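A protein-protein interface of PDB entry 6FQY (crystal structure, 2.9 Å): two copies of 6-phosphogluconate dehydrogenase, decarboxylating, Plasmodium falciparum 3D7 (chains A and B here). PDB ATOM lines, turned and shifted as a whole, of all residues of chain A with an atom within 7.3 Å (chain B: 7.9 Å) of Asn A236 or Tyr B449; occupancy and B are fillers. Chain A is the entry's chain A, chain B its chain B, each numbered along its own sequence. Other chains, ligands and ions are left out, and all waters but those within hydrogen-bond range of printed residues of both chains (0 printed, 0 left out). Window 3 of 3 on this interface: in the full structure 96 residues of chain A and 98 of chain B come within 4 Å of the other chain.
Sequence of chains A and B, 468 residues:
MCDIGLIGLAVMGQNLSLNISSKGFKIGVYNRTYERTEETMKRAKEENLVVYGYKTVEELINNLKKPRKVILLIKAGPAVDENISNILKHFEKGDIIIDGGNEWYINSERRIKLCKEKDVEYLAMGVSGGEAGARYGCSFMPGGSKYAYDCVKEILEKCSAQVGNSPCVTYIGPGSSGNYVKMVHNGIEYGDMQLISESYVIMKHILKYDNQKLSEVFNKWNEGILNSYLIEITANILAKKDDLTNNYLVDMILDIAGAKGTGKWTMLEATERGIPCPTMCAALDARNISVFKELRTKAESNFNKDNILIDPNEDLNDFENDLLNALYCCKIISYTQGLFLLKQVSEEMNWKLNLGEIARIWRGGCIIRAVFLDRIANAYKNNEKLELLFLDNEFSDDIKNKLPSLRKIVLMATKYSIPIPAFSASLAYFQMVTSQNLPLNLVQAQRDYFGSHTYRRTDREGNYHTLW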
ATOM      1  N   GLU A 131     -25.677  32.923  22.651  1.00  0.00           N
ATOM      2  CA  GLU A 131     -25.357  34.269  23.093  1.00  0.00           C
ATOM      3  C   GLU A 131     -26.306  35.329  22.551  1.00  0.00           C
ATOM      4  O   GLU A 131     -26.259  36.477  23.014  1.00  0.00           O
ATOM      5  CB  GLU A 131     -23.935  34.610  22.631  1.00  0.00           C
ATOM      6  CG  GLU A 131     -23.734  34.662  21.088  1.00  0.00           C
ATOM      7  CD  GLU A 131     -23.985  33.348  20.329  1.00  0.00           C
ATOM      8  OE1 GLU A 131     -24.267  32.302  20.947  1.00  0.00           O
ATOM      9  OE2 GLU A 131     -23.904  33.368  19.083  1.00  0.00           O
ATOM     10  N   ALA A 132     -27.164  34.974  21.593  1.00  0.00           N
ATOM     11  CA  ALA A 132     -28.336  35.790  21.304  1.00  0.00           C
ATOM     12  C   ALA A 132     -29.425  35.563  22.344  1.00  0.00           C
ATOM     13  O   ALA A 132     -29.972  36.519  22.903  1.00  0.00           O
ATOM     14  CB  ALA A 132     -28.853  35.479  19.901  1.00  0.00           C
ATOM     15  N   SER A 215     -32.035  28.170  -0.848  1.00  0.00           N
ATOM     16  CA  SER A 215     -32.361  29.174   0.157  1.00  0.00           C
ATOM     17  C   SER A 215     -33.825  29.588   0.081  1.00  0.00           C
ATOM     18  O   SER A 215     -34.442  29.886   1.110  1.00  0.00           O
ATOM     19  CB  SER A 215     -31.458  30.396  -0.012  1.00  0.00           C
ATOM     20  OG  SER A 215     -31.765  31.393   0.946  1.00  0.00           O
ATOM     21  N   PHE A 218     -36.049  26.765   1.561  1.00  0.00           N
ATOM     22  CA  PHE A 218     -35.974  26.813   3.017  1.00  0.00           C
ATOM     23  C   PHE A 218     -36.693  28.045   3.550  1.00  0.00           C
ATOM     24  O   PHE A 218     -37.341  27.986   4.604  1.00  0.00           O
ATOM     25  CB  PHE A 218     -34.516  26.782   3.471  1.00  0.00           C
ATOM     26  CG  PHE A 218     -33.933  25.396   3.544  1.00  0.00           C
ATOM     27  CD1 PHE A 218     -34.415  24.471   4.457  1.00  0.00           C
ATOM     28  CD2 PHE A 218     -32.900  25.019   2.702  1.00  0.00           C
ATOM     29  CE1 PHE A 218     -33.873  23.194   4.529  1.00  0.00           C
ATOM     30  CE2 PHE A 218     -32.355  23.741   2.769  1.00  0.00           C
ATOM     31  CZ  PHE A 218     -32.843  22.830   3.684  1.00  0.00           C
ATOM     32  N   ASN A 219     -36.603  29.168   2.830  1.00  0.00           N
ATOM     33  CA  ASN A 219     -37.411  30.324   3.201  1.00  0.00           C
ATOM     34  C   ASN A 219     -38.902  30.072   2.929  1.00  0.00           C
ATOM     35  O   ASN A 219     -39.747  30.714   3.550  1.00  0.00           O
ATOM     36  CB  ASN A 219     -36.898  31.587   2.493  1.00  0.00           C
ATOM     37  CG  ASN A 219     -36.056  32.490   3.424  1.00  0.00           C
ATOM     38  OD1 ASN A 219     -36.385  32.655   4.600  1.00  0.00           O
ATOM     39  ND2 ASN A 219     -34.976  33.073   2.894  1.00  0.00           N
ATOM     40  N   TYR A 229     -36.146  27.815  13.949  1.00  0.00           N
ATOM     41  CA  TYR A 229     -34.941  28.631  13.910  1.00  0.00           C
ATOM     42  C   TYR A 229     -33.908  28.045  12.957  1.00  0.00           C
ATOM     43  O   TYR A 229     -33.262  28.782  12.206  1.00  0.00           O
ATOM     44  CB  TYR A 229     -34.347  28.772  15.311  1.00  0.00           C
ATOM     45  CG  TYR A 229     -32.987  29.436  15.322  1.00  0.00           C
ATOM     46  CD1 TYR A 229     -31.842  28.706  15.618  1.00  0.00           C
ATOM     47  CD2 TYR A 229     -32.844  30.784  15.025  1.00  0.00           C
ATOM     48  CE1 TYR A 229     -30.596  29.300  15.625  1.00  0.00           C
ATOM     49  CE2 TYR A 229     -31.602  31.388  15.031  1.00  0.00           C
ATOM     50  CZ  TYR A 229     -30.482  30.640  15.331  1.00  0.00           C
ATOM     51  OH  TYR A 229     -29.243  31.238  15.336  1.00  0.00           O
ATOM     52  N   LEU A 230     -33.751  26.720  12.955  1.00  0.00           N
ATOM     53  CA  LEU A 230     -32.711  26.114  12.132  1.00  0.00           C
ATOM     54  C   LEU A 230     -33.053  26.200  10.650  1.00  0.00           C
ATOM     55  O   LEU A 230     -32.167  26.409   9.815  1.00  0.00           O
ATOM     56  CB  LEU A 230     -32.508  24.655  12.525  1.00  0.00           C
ATOM     57  CG  LEU A 230     -32.204  24.407  14.003  1.00  0.00           C
ATOM     58  CD1 LEU A 230     -33.477  23.844  14.667  1.00  0.00           C
ATOM     59  CD2 LEU A 230     -30.992  23.521  14.224  1.00  0.00           C
ATOM     60  N   ILE A 231     -34.329  26.026  10.300  1.00  0.00           N
ATOM     61  CA  ILE A 231     -34.729  26.093   8.896  1.00  0.00           C
ATOM     62  C   ILE A 231     -34.483  27.489   8.332  1.00  0.00           C
ATOM     63  O   ILE A 231     -34.037  27.642   7.187  1.00  0.00           O
ATOM     64  CB  ILE A 231     -36.200  25.649   8.731  1.00  0.00           C
ATOM     65  CG1 ILE A 231     -36.329  24.137   8.904  1.00  0.00           C
ATOM     66  CG2 ILE A 231     -36.747  26.077   7.401  1.00  0.00           C
ATOM     67  CD1 ILE A 231     -35.906  23.355   7.671  1.00  0.00           C
ATOM     68  N   GLU A 232     -34.749  28.528   9.124  1.00  0.00           N
ATOM     69  CA  GLU A 232     -34.590  29.883   8.609  1.00  0.00           C
ATOM     70  C   GLU A 232     -33.118  30.237   8.434  1.00  0.00           C
ATOM     71  O   GLU A 232     -32.760  30.951   7.491  1.00  0.00           O
ATOM     72  CB  GLU A 232     -35.313  30.883   9.514  1.00  0.00           C
ATOM     73  CG  GLU A 232     -34.493  31.490  10.633  1.00  0.00           C
ATOM     74  CD  GLU A 232     -35.174  32.692  11.250  1.00  0.00           C
ATOM     75  OE1 GLU A 232     -36.260  32.520  11.843  1.00  0.00           O
ATOM     76  OE2 GLU A 232     -34.629  33.811  11.135  1.00  0.00           O
ATOM     77  N   ILE A 233     -32.247  29.743   9.319  1.00  0.00           N
ATOM     78  CA  ILE A 233     -30.834  30.091   9.202  1.00  0.00           C
ATOM     79  C   ILE A 233     -30.175  29.356   8.039  1.00  0.00           C
ATOM     80  O   ILE A 233     -29.195  29.851   7.470  1.00  0.00           O
ATOM     81  CB  ILE A 233     -30.096  29.845  10.534  1.00  0.00           C
ATOM     82  CG1 ILE A 233     -29.981  28.353  10.850  1.00  0.00           C
ATOM     83  CG2 ILE A 233     -30.777  30.596  11.666  1.00  0.00           C
ATOM     84  CD1 ILE A 233     -28.858  28.027  11.815  1.00  0.00           C
ATOM     85  N   THR A 234     -30.683  28.177   7.653  1.00  0.00           N
ATOM     86  CA  THR A 234     -30.148  27.526   6.457  1.00  0.00           C
ATOM     87  C   THR A 234     -30.460  28.341   5.211  1.00  0.00           C
ATOM     88  O   THR A 234     -29.629  28.439   4.301  1.00  0.00           O
ATOM     89  CB  THR A 234     -30.710  26.114   6.290  1.00  0.00           C
ATOM     90  OG1 THR A 234     -32.073  26.187   5.855  1.00  0.00           O
ATOM     91  CG2 THR A 234     -30.634  25.346   7.574  1.00  0.00           C
ATOM     92  N   ALA A 235     -31.659  28.924   5.151  1.00  0.00           N
ATOM     93  CA  ALA A 235     -31.998  29.815   4.048  1.00  0.00           C
ATOM     94  C   ALA A 235     -31.028  30.986   3.978  1.00  0.00           C
ATOM     95  O   ALA A 235     -30.637  31.415   2.887  1.00  0.00           O
ATOM     96  CB  ALA A 235     -33.435  30.309   4.197  1.00  0.00           C
ATOM     97  N   ASN A 236     -30.631  31.518   5.135  1.00  0.00           N
ATOM     98  CA  ASN A 236     -29.639  32.586   5.152  1.00  0.00           C
ATOM     99  C   ASN A 236     -28.258  32.062   4.774  1.00  0.00           C
ATOM    100  O   ASN A 236     -27.521  32.720   4.030  1.00  0.00           O
ATOM    101  CB  ASN A 236     -29.607  33.248   6.528  1.00  0.00           C
ATOM    102  CG  ASN A 236     -30.957  33.799   6.940  1.00  0.00           C
ATOM    103  OD1 ASN A 236     -31.861  33.941   6.116  1.00  0.00           O
ATOM    104  ND2 ASN A 236     -31.102  34.114   8.222  1.00  0.00           N
ATOM    105  N   ILE A 237     -27.890  30.882   5.281  1.00  0.00           N
ATOM    106  CA  ILE A 237     -26.561  30.332   5.021  1.00  0.00           C
ATOM    107  C   ILE A 237     -26.382  30.032   3.538  1.00  0.00           C
ATOM    108  O   ILE A 237     -25.360  30.382   2.934  1.00  0.00           O
ATOM    109  CB  ILE A 237     -26.317  29.079   5.880  1.00  0.00           C
ATOM    110  CG1 ILE A 237     -26.004  29.467   7.328  1.00  0.00           C
ATOM    111  CG2 ILE A 237     -25.203  28.231   5.288  1.00  0.00           C
ATOM    112  CD1 ILE A 237     -26.458  28.442   8.348  1.00  0.00           C
ATOM    113  N   LEU A 238     -27.374  29.380   2.926  1.00  0.00           N
ATOM    114  CA  LEU A 238     -27.247  28.970   1.532  1.00  0.00           C
ATOM    115  C   LEU A 238     -27.181  30.155   0.575  1.00  0.00           C
ATOM    116  O   LEU A 238     -26.670  30.003  -0.539  1.00  0.00           O
ATOM    117  CB  LEU A 238     -28.405  28.045   1.155  1.00  0.00           C
ATOM    118  CG  LEU A 238     -28.381  26.693   1.875  1.00  0.00           C
ATOM    119  CD1 LEU A 238     -29.630  25.884   1.580  1.00  0.00           C
ATOM    120  CD2 LEU A 238     -27.132  25.911   1.501  1.00  0.00           C
ATOM    121  N   ALA A 239     -27.686  31.320   0.976  1.00  0.00           N
ATOM    122  CA  ALA A 239     -27.622  32.520   0.154  1.00  0.00           C
ATOM    123  C   ALA A 239     -26.381  33.364   0.418  1.00  0.00           C
ATOM    124  O   ALA A 239     -26.082  34.263  -0.376  1.00  0.00           O
ATOM    125  CB  ALA A 239     -28.872  33.378   0.373  1.00  0.00           C
ATOM    126  N   LYS A 240     -25.656  33.092   1.500  1.00  0.00           N
ATOM    127  CA  LYS A 240     -24.525  33.924   1.891  1.00  0.00           C
ATOM    128  C   LYS A 240     -23.383  33.826   0.890  1.00  0.00           C
ATOM    129  O   LYS A 240     -23.057  32.745   0.391  1.00  0.00           O
ATOM    130  CB  LYS A 240     -24.029  33.530   3.282  1.00  0.00           C
ATOM    131  CG  LYS A 240     -22.933  34.438   3.822  1.00  0.00           C
ATOM    132  CD  LYS A 240     -23.497  35.748   4.344  1.00  0.00           C
ATOM    133  CE  LYS A 240     -22.386  36.749   4.617  1.00  0.00           C
ATOM    134  NZ  LYS A 240     -22.915  38.063   5.077  1.00  0.00           N
ATOM    135  N   LYS A 241     -22.775  34.970   0.600  1.00  0.00           N
ATOM    136  CA  LYS A 241     -21.675  35.057  -0.347  1.00  0.00           C
ATOM    137  C   LYS A 241     -20.348  35.138   0.394  1.00  0.00           C
ATOM    138  O   LYS A 241     -20.238  35.799   1.433  1.00  0.00           O
ATOM    139  CB  LYS A 241     -21.842  36.285  -1.248  1.00  0.00           C
ATOM    140  CG  LYS A 241     -20.701  36.528  -2.233  1.00  0.00           C
ATOM    141  CD  LYS A 241     -20.870  37.858  -2.965  1.00  0.00           C
ATOM    142  CE  LYS A 241     -20.495  39.042  -2.080  1.00  0.00           C
ATOM    143  NZ  LYS A 241     -21.060  40.326  -2.589  1.00  0.00           N
ATOM    144  N   LEU B 442     -22.889  22.519   5.602  1.00  0.00           N
ATOM    145  CA  LEU B 442     -24.057  23.224   6.118  1.00  0.00           C
ATOM    146  C   LEU B 442     -24.130  23.135   7.635  1.00  0.00           C
ATOM    147  O   LEU B 442     -24.598  24.073   8.292  1.00  0.00           O
ATOM    148  CB  LEU B 442     -25.330  22.652   5.486  1.00  0.00           C
ATOM    149  CG  LEU B 442     -26.658  23.328   5.832  1.00  0.00           C
ATOM    150  CD1 LEU B 442     -26.559  24.828   5.627  1.00  0.00           C
ATOM    151  CD2 LEU B 442     -27.792  22.740   5.004  1.00  0.00           C
ATOM    152  N   VAL B 443     -23.676  22.018   8.208  1.00  0.00           N
ATOM    153  CA  VAL B 443     -23.660  21.871   9.660  1.00  0.00           C
ATOM    154  C   VAL B 443     -22.644  22.822  10.282  1.00  0.00           C
ATOM    155  O   VAL B 443     -22.939  23.518  11.260  1.00  0.00           O
ATOM    156  CB  VAL B 443     -23.374  20.408  10.045  1.00  0.00           C
ATOM    157  CG1 VAL B 443     -23.119  20.288  11.538  1.00  0.00           C
ATOM    158  CG2 VAL B 443     -24.531  19.516   9.626  1.00  0.00           C
ATOM    159  N   GLN B 444     -21.430  22.864   9.723  1.00  0.00           N
ATOM    160  CA  GLN B 444     -20.408  23.775  10.233  1.00  0.00           C
ATOM    161  C   GLN B 444     -20.844  25.228  10.103  1.00  0.00           C
ATOM    162  O   GLN B 444     -20.537  26.056  10.970  1.00  0.00           O
ATOM    163  CB  GLN B 444     -19.088  23.545   9.496  1.00  0.00           C
ATOM    164  CG  GLN B 444     -18.274  22.380  10.027  1.00  0.00           C
ATOM    165  CD  GLN B 444     -17.722  22.643  11.414  1.00  0.00           C
ATOM    166  OE1 GLN B 444     -18.333  22.279  12.419  1.00  0.00           O
ATOM    167  NE2 GLN B 444     -16.560  23.281  11.475  1.00  0.00           N
ATOM    168  N   ALA B 445     -21.554  25.558   9.024  1.00  0.00           N
ATOM    169  CA  ALA B 445     -22.069  26.914   8.869  1.00  0.00           C
ATOM    170  C   ALA B 445     -23.145  27.215   9.904  1.00  0.00           C
ATOM    171  O   ALA B 445     -23.255  28.350  10.383  1.00  0.00           O
ATOM    172  CB  ALA B 445     -22.611  27.106   7.454  1.00  0.00           C
ATOM    173  N   GLN B 446     -23.946  26.208  10.257  1.00  0.00           N
ATOM    174  CA  GLN B 446     -24.984  26.399  11.264  1.00  0.00           C
ATOM    175  C   GLN B 446     -24.377  26.623  12.643  1.00  0.00           C
ATOM    176  O   GLN B 446     -24.788  27.532  13.371  1.00  0.00           O
ATOM    177  CB  GLN B 446     -25.917  25.190  11.278  1.00  0.00           C
ATOM    178  CG  GLN B 446     -26.960  25.199  10.181  1.00  0.00           C
ATOM    179  CD  GLN B 446     -27.448  23.804   9.853  1.00  0.00           C
ATOM    180  OE1 GLN B 446     -26.955  22.820  10.400  1.00  0.00           O
ATOM    181  NE2 GLN B 446     -28.402  23.708   8.943  1.00  0.00           N
ATOM    182  N   ARG B 447     -23.393  25.801  13.020  1.00  0.00           N
ATOM    183  CA  ARG B 447     -22.791  25.939  14.343  1.00  0.00           C
ATOM    184  C   ARG B 447     -22.095  27.286  14.493  1.00  0.00           C
ATOM    185  O   ARG B 447     -22.112  27.884  15.575  1.00  0.00           O
ATOM    186  CB  ARG B 447     -21.815  24.792  14.605  1.00  0.00           C
ATOM    187  CG  ARG B 447     -22.450  23.413  14.564  1.00  0.00           C
ATOM    188  CD  ARG B 447     -21.595  22.408  15.312  1.00  0.00           C
ATOM    189  NE  ARG B 447     -20.184  22.783  15.285  1.00  0.00           N
ATOM    190  CZ  ARG B 447     -19.270  22.323  16.132  1.00  0.00           C
ATOM    191  NH1 ARG B 447     -19.614  21.459  17.077  1.00  0.00           N
ATOM    192  NH2 ARG B 447     -18.010  22.721  16.030  1.00  0.00           N
ATOM    193  N   ASP B 448     -21.475  27.779  13.419  1.00  0.00           N
ATOM    194  CA  ASP B 448     -20.897  29.116  13.464  1.00  0.00           C
ATOM    195  C   ASP B 448     -21.984  30.179  13.540  1.00  0.00           C
ATOM    196  O   ASP B 448     -21.754  31.265  14.083  1.00  0.00           O
ATOM    197  CB  ASP B 448     -20.005  29.346  12.242  1.00  0.00           C
ATOM    198  CG  ASP B 448     -19.284  30.681  12.287  1.00  0.00           C
ATOM    199  OD1 ASP B 448     -18.369  30.837  13.122  1.00  0.00           O
ATOM    200  OD2 ASP B 448     -19.630  31.573  11.484  1.00  0.00           O
ATOM    201  N   TYR B 449     -23.167  29.883  12.997  1.00  0.00           N
ATOM    202  CA  TYR B 449     -24.280  30.826  13.033  1.00  0.00           C
ATOM    203  C   TYR B 449     -24.757  31.065  14.463  1.00  0.00           C
ATOM    204  O   TYR B 449     -24.726  32.196  14.960  1.00  0.00           O
ATOM    205  CB  TYR B 449     -25.423  30.299  12.158  1.00  0.00           C
ATOM    206  CG  TYR B 449     -26.447  31.327  11.724  1.00  0.00           C
ATOM    207  CD1 TYR B 449     -27.270  31.955  12.650  1.00  0.00           C
ATOM    208  CD2 TYR B 449     -26.613  31.643  10.381  1.00  0.00           C
ATOM    209  CE1 TYR B 449     -28.212  32.885  12.256  1.00  0.00           C
ATOM    210  CE2 TYR B 449     -27.555  32.571   9.977  1.00  0.00           C
ATOM    211  CZ  TYR B 449     -28.352  33.187  10.919  1.00  0.00           C
ATOM    212  OH  TYR B 449     -29.291  34.111  10.521  1.00  0.00           O
ATOM    213  N   PHE B 450     -25.198  30.004  15.146  1.00  0.00           N
ATOM    214  CA  PHE B 450     -25.825  30.154  16.454  1.00  0.00           C
ATOM    215  C   PHE B 450     -24.866  29.970  17.623  1.00  0.00           C
ATOM    216  O   PHE B 450     -25.170  30.434  18.728  1.00  0.00           O
ATOM    217  CB  PHE B 450     -27.013  29.188  16.601  1.00  0.00           C
ATOM    218  CG  PHE B 450     -26.661  27.731  16.421  1.00  0.00           C
ATOM    219  CD1 PHE B 450     -26.010  27.021  17.421  1.00  0.00           C
ATOM    220  CD2 PHE B 450     -27.026  27.058  15.267  1.00  0.00           C
ATOM    221  CE1 PHE B 450     -25.700  25.684  17.255  1.00  0.00           C
ATOM    222  CE2 PHE B 450     -26.719  25.720  15.096  1.00  0.00           C
ATOM    223  CZ  PHE B 450     -26.056  25.033  16.092  1.00  0.00           C
ATOM    224  N   GLY B 451     -23.727  29.314  17.418  1.00  0.00           N
ATOM    225  CA  GLY B 451     -22.845  28.997  18.527  1.00  0.00           C
ATOM    226  C   GLY B 451     -21.482  29.645  18.401  1.00  0.00           C
ATOM    227  O   GLY B 451     -20.655  29.561  19.315  1.00  0.00           O
ATOM    228  N   SER B 452     -21.247  30.294  17.261  1.00  0.00           N
ATOM    229  CA  SER B 452     -19.990  30.986  16.969  1.00  0.00           C
ATOM    230  C   SER B 452     -18.786  30.051  17.070  1.00  0.00           C
ATOM    231  O   SER B 452     -17.702  30.449  17.502  1.00  0.00           O
ATOM    232  CB  SER B 452     -19.810  32.204  17.877  1.00  0.00           C
ATOM    233  OG  SER B 452     -20.915  33.084  17.777  1.00  0.00           O
ATOM    234  N   HIS B 453     -18.977  28.794  16.678  1.00  0.00           N
ATOM    235  CA  HIS B 453     -17.866  27.856  16.589  1.00  0.00           C
ATOM    236  C   HIS B 453     -17.086  28.122  15.308  1.00  0.00           C
ATOM    237  O   HIS B 453     -17.675  28.271  14.234  1.00  0.00           O
ATOM    238  CB  HIS B 453     -18.361  26.410  16.624  1.00  0.00           C
ATOM    239  CG  HIS B 453     -19.115  26.058  17.867  1.00  0.00           C
ATOM    240  ND1 HIS B 453     -20.467  26.287  18.009  1.00  0.00           N
ATOM    241  CD2 HIS B 453     -18.706  25.489  19.026  1.00  0.00           C
ATOM    242  CE1 HIS B 453     -20.858  25.875  19.202  1.00  0.00           C
ATOM    243  NE2 HIS B 453     -19.808  25.387  19.839  1.00  0.00           N
ATOM    244  N   TYR B 455     -14.652  27.673  11.992  1.00  0.00           N
ATOM    245  CA  TYR B 455     -14.663  26.683  10.926  1.00  0.00           C
ATOM    246  C   TYR B 455     -13.418  26.846  10.063  1.00  0.00           C
ATOM    247  O   TYR B 455     -12.757  27.887  10.076  1.00  0.00           O
ATOM    248  CB  TYR B 455     -15.935  26.783  10.059  1.00  0.00           C
ATOM    249  CG  TYR B 455     -16.079  28.050   9.231  1.00  0.00           C
ATOM    250  CD1 TYR B 455     -16.736  29.167   9.733  1.00  0.00           C
ATOM    251  CD2 TYR B 455     -15.588  28.111   7.932  1.00  0.00           C
ATOM    252  CE1 TYR B 455     -16.877  30.316   8.971  1.00  0.00           C
ATOM    253  CE2 TYR B 455     -15.724  29.254   7.164  1.00  0.00           C
ATOM    254  CZ  TYR B 455     -16.369  30.353   7.688  1.00  0.00           C
ATOM    255  OH  TYR B 455     -16.505  31.489   6.923  1.00  0.00           O
ATOM    256  N   HIS B 465     -14.648  32.917  11.371  1.00  0.00           N
ATOM    257  CA  HIS B 465     -15.982  33.168  11.894  1.00  0.00           C
ATOM    258  C   HIS B 465     -16.647  34.198  10.995  1.00  0.00           C
ATOM    259  O   HIS B 465     -15.989  35.126  10.516  1.00  0.00           O
ATOM    260  CB  HIS B 465     -15.944  33.669  13.344  1.00  0.00           C
ATOM    261  CG  HIS B 465     -17.259  34.190  13.837  1.00  0.00           C
ATOM    262  ND1 HIS B 465     -18.376  33.392  13.959  1.00  0.00           N
ATOM    263  CD2 HIS B 465     -17.635  35.427  14.238  1.00  0.00           C
ATOM    264  CE1 HIS B 465     -19.384  34.115  14.413  1.00  0.00           C
ATOM    265  NE2 HIS B 465     -18.960  35.354  14.592  1.00  0.00           N
ATOM    266  N   THR B 466     -17.945  34.034  10.762  1.00  0.00           N
ATOM    267  CA  THR B 466     -18.654  34.880   9.816  1.00  0.00           C
ATOM    268  C   THR B 466     -19.865  35.517  10.479  1.00  0.00           C
ATOM    269  O   THR B 466     -20.569  34.874  11.263  1.00  0.00           O
ATOM    270  CB  THR B 466     -19.107  34.067   8.588  1.00  0.00           C
ATOM    271  OG1 THR B 466     -17.960  33.637   7.845  1.00  0.00           O
ATOM    272  CG2 THR B 466     -20.011  34.896   7.683  1.00  0.00           C
ATOM    273  N   LEU B 467     -20.086  36.792  10.169  1.00  0.00           N
ATOM    274  CA  LEU B 467     -21.331  37.478  10.502  1.00  0.00           C
ATOM    275  C   LEU B 467     -22.283  37.187   9.349  1.00  0.00           C
ATOM    276  O   LEU B 467     -22.233  37.844   8.307  1.00  0.00           O
ATOM    277  CB  LEU B 467     -21.101  38.974  10.691  1.00  0.00           C
ATOM    278  CG  LEU B 467     -20.393  39.508  11.947  1.00  0.00           C
ATOM    279  CD1 LEU B 467     -18.997  38.920  12.146  1.00  0.00           C
ATOM    280  CD2 LEU B 467     -20.319  41.028  11.902  1.00  0.00           C
ATOM    281  N   TRP B 468     -23.154  36.202   9.533  1.00  0.00           N
ATOM    282  CA  TRP B 468     -23.994  35.723   8.441  1.00  0.00           C
ATOM    283  C   TRP B 468     -25.120  36.703   8.129  1.00  0.00           C
ATOM    284  O   TRP B 468     -25.840  36.542   7.144  1.00  0.00           O
ATOM    285  CB  TRP B 468     -24.567  34.342   8.773  1.00  0.00           C
ATOM    286  CG  TRP B 468     -23.522  33.358   9.219  1.00  0.00           C
ATOM    287  CD1 TRP B 468     -22.995  33.239  10.472  1.00  0.00           C
ATOM    288  CD2 TRP B 468     -22.858  32.375   8.411  1.00  0.00           C
ATOM    289  NE1 TRP B 468     -22.057  32.236  10.499  1.00  0.00           N
ATOM    290  CE2 TRP B 468     -21.953  31.691   9.247  1.00  0.00           C
ATOM    291  CE3 TRP B 468     -22.947  32.004   7.066  1.00  0.00           C
ATOM    292  CZ2 TRP B 468     -21.143  30.657   8.782  1.00  0.00           C
ATOM    293  CZ3 TRP B 468     -22.141  30.976   6.608  1.00  0.00           C
ATOM    294  CH2 TRP B 468     -21.249  30.317   7.463  1.00  0.00           C
ATOM    295  OXT TRP B 468     -25.333  37.679   8.848  1.00  0.00           O
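The side-chain carboxylate (OE2) of Glu A131 sits at hydrogen-bond distance from the side-chain hydroxyl (OG) of Ser B452.
OH of Tyr B449 sits at hydrogen-bond distance from ND2 of Asn A236 (2.9 Å).
The side-chain amino group of Lys A240 is in hydrogen-bond range of the backbone carbonyl oxygen of Leu B467, at 3.3 Å.
NZ of Lys A240 lies within salt-bridge range of O of Trp B468, at 3.9 Å.
OE1 of Glu A131 lies close to O of Phe B450 (3.0 Å).
The side-chain hydroxyl (OG1) of Thr A234 sits at hydrogen-bond distance from the backbone carbonyl oxygen (O) of Ile A231 (2.8 Å).
The backbone carbonyl oxygen (O) of Glu A232 lies close to the side-chain amide oxygen (OD1) of Asn A236, 3.4 Å away.
The backbone carbonyl oxygen (O) of Leu B442 sits close to the side-chain amide oxygen (OE1) of Gln B446 (3.4 Å).
O of Arg B447 sits at hydrogen-bond distance from N of Ser B452.
OD2 of Asp B448 lies within hydrogen-bond range of NE1 of Trp B468 (2.7 Å).
The indole nitrogen (NE1) of Trp B468 lies close to the backbone carbonyl oxygen (O) of Thr B466, at 3.1 Å.
Among the printed residues, merely in contact across the chains: Thr A234 with Gln B446 (3.1 Å), Tyr A229 with Phe B450 (3.3 Å), Tyr A229 with Tyr B449 (3.4 Å), Ile A233 with Tyr B449 (3.5 Å), Ile A237 with Ala B445 (3.6 Å), Ile A237 with Leu B442 (3.7 Å), Ile A237 with Gln B446 (3.8 Å), Ile A233 with Gln B446 (3.8 Å), Ile A237 with Tyr B449 (3.8 Å) and Ile A237 with Trp B468 (3.98 Å).
Of the printed residues of chain B, Tyr A229 touches Tyr B449 (3.4 Å) and Phe B450 (3.3 Å).
Of chain B, only Tyr B449 comes within 4 Å of Asn A236.
Of the printed residues of chain A, Leu B442 touches Ile A237 (3.7 Å).
Of chain A, only Tyr A229 (3.4 Å), Ile A233 (3.5 Å), Asn A236 (2.9 Å) and Ile A237 (3.8 Å) come within 4 Å of Tyr B449.
The nearest residue of chain A that does not touch Tyr B449 is Glu A131 (4.4 Å).
Of the 18 printed residues of chain A, 7 touch a printed residue of chain B.
Of the 17 printed residues of chain B, 8 touch a printed residue of chain A.
Hydrophobic or aromatic side chains of chain B that line the printed part of chain A: Leu B442, Ala B445, Tyr B449, Phe B450 and Trp B468.
Among the printed residues, no Asp or Glu carboxylate lies within 4 Å of a Lys or Arg side-chain nitrogen of the other chain.
No position is printed for both chains.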
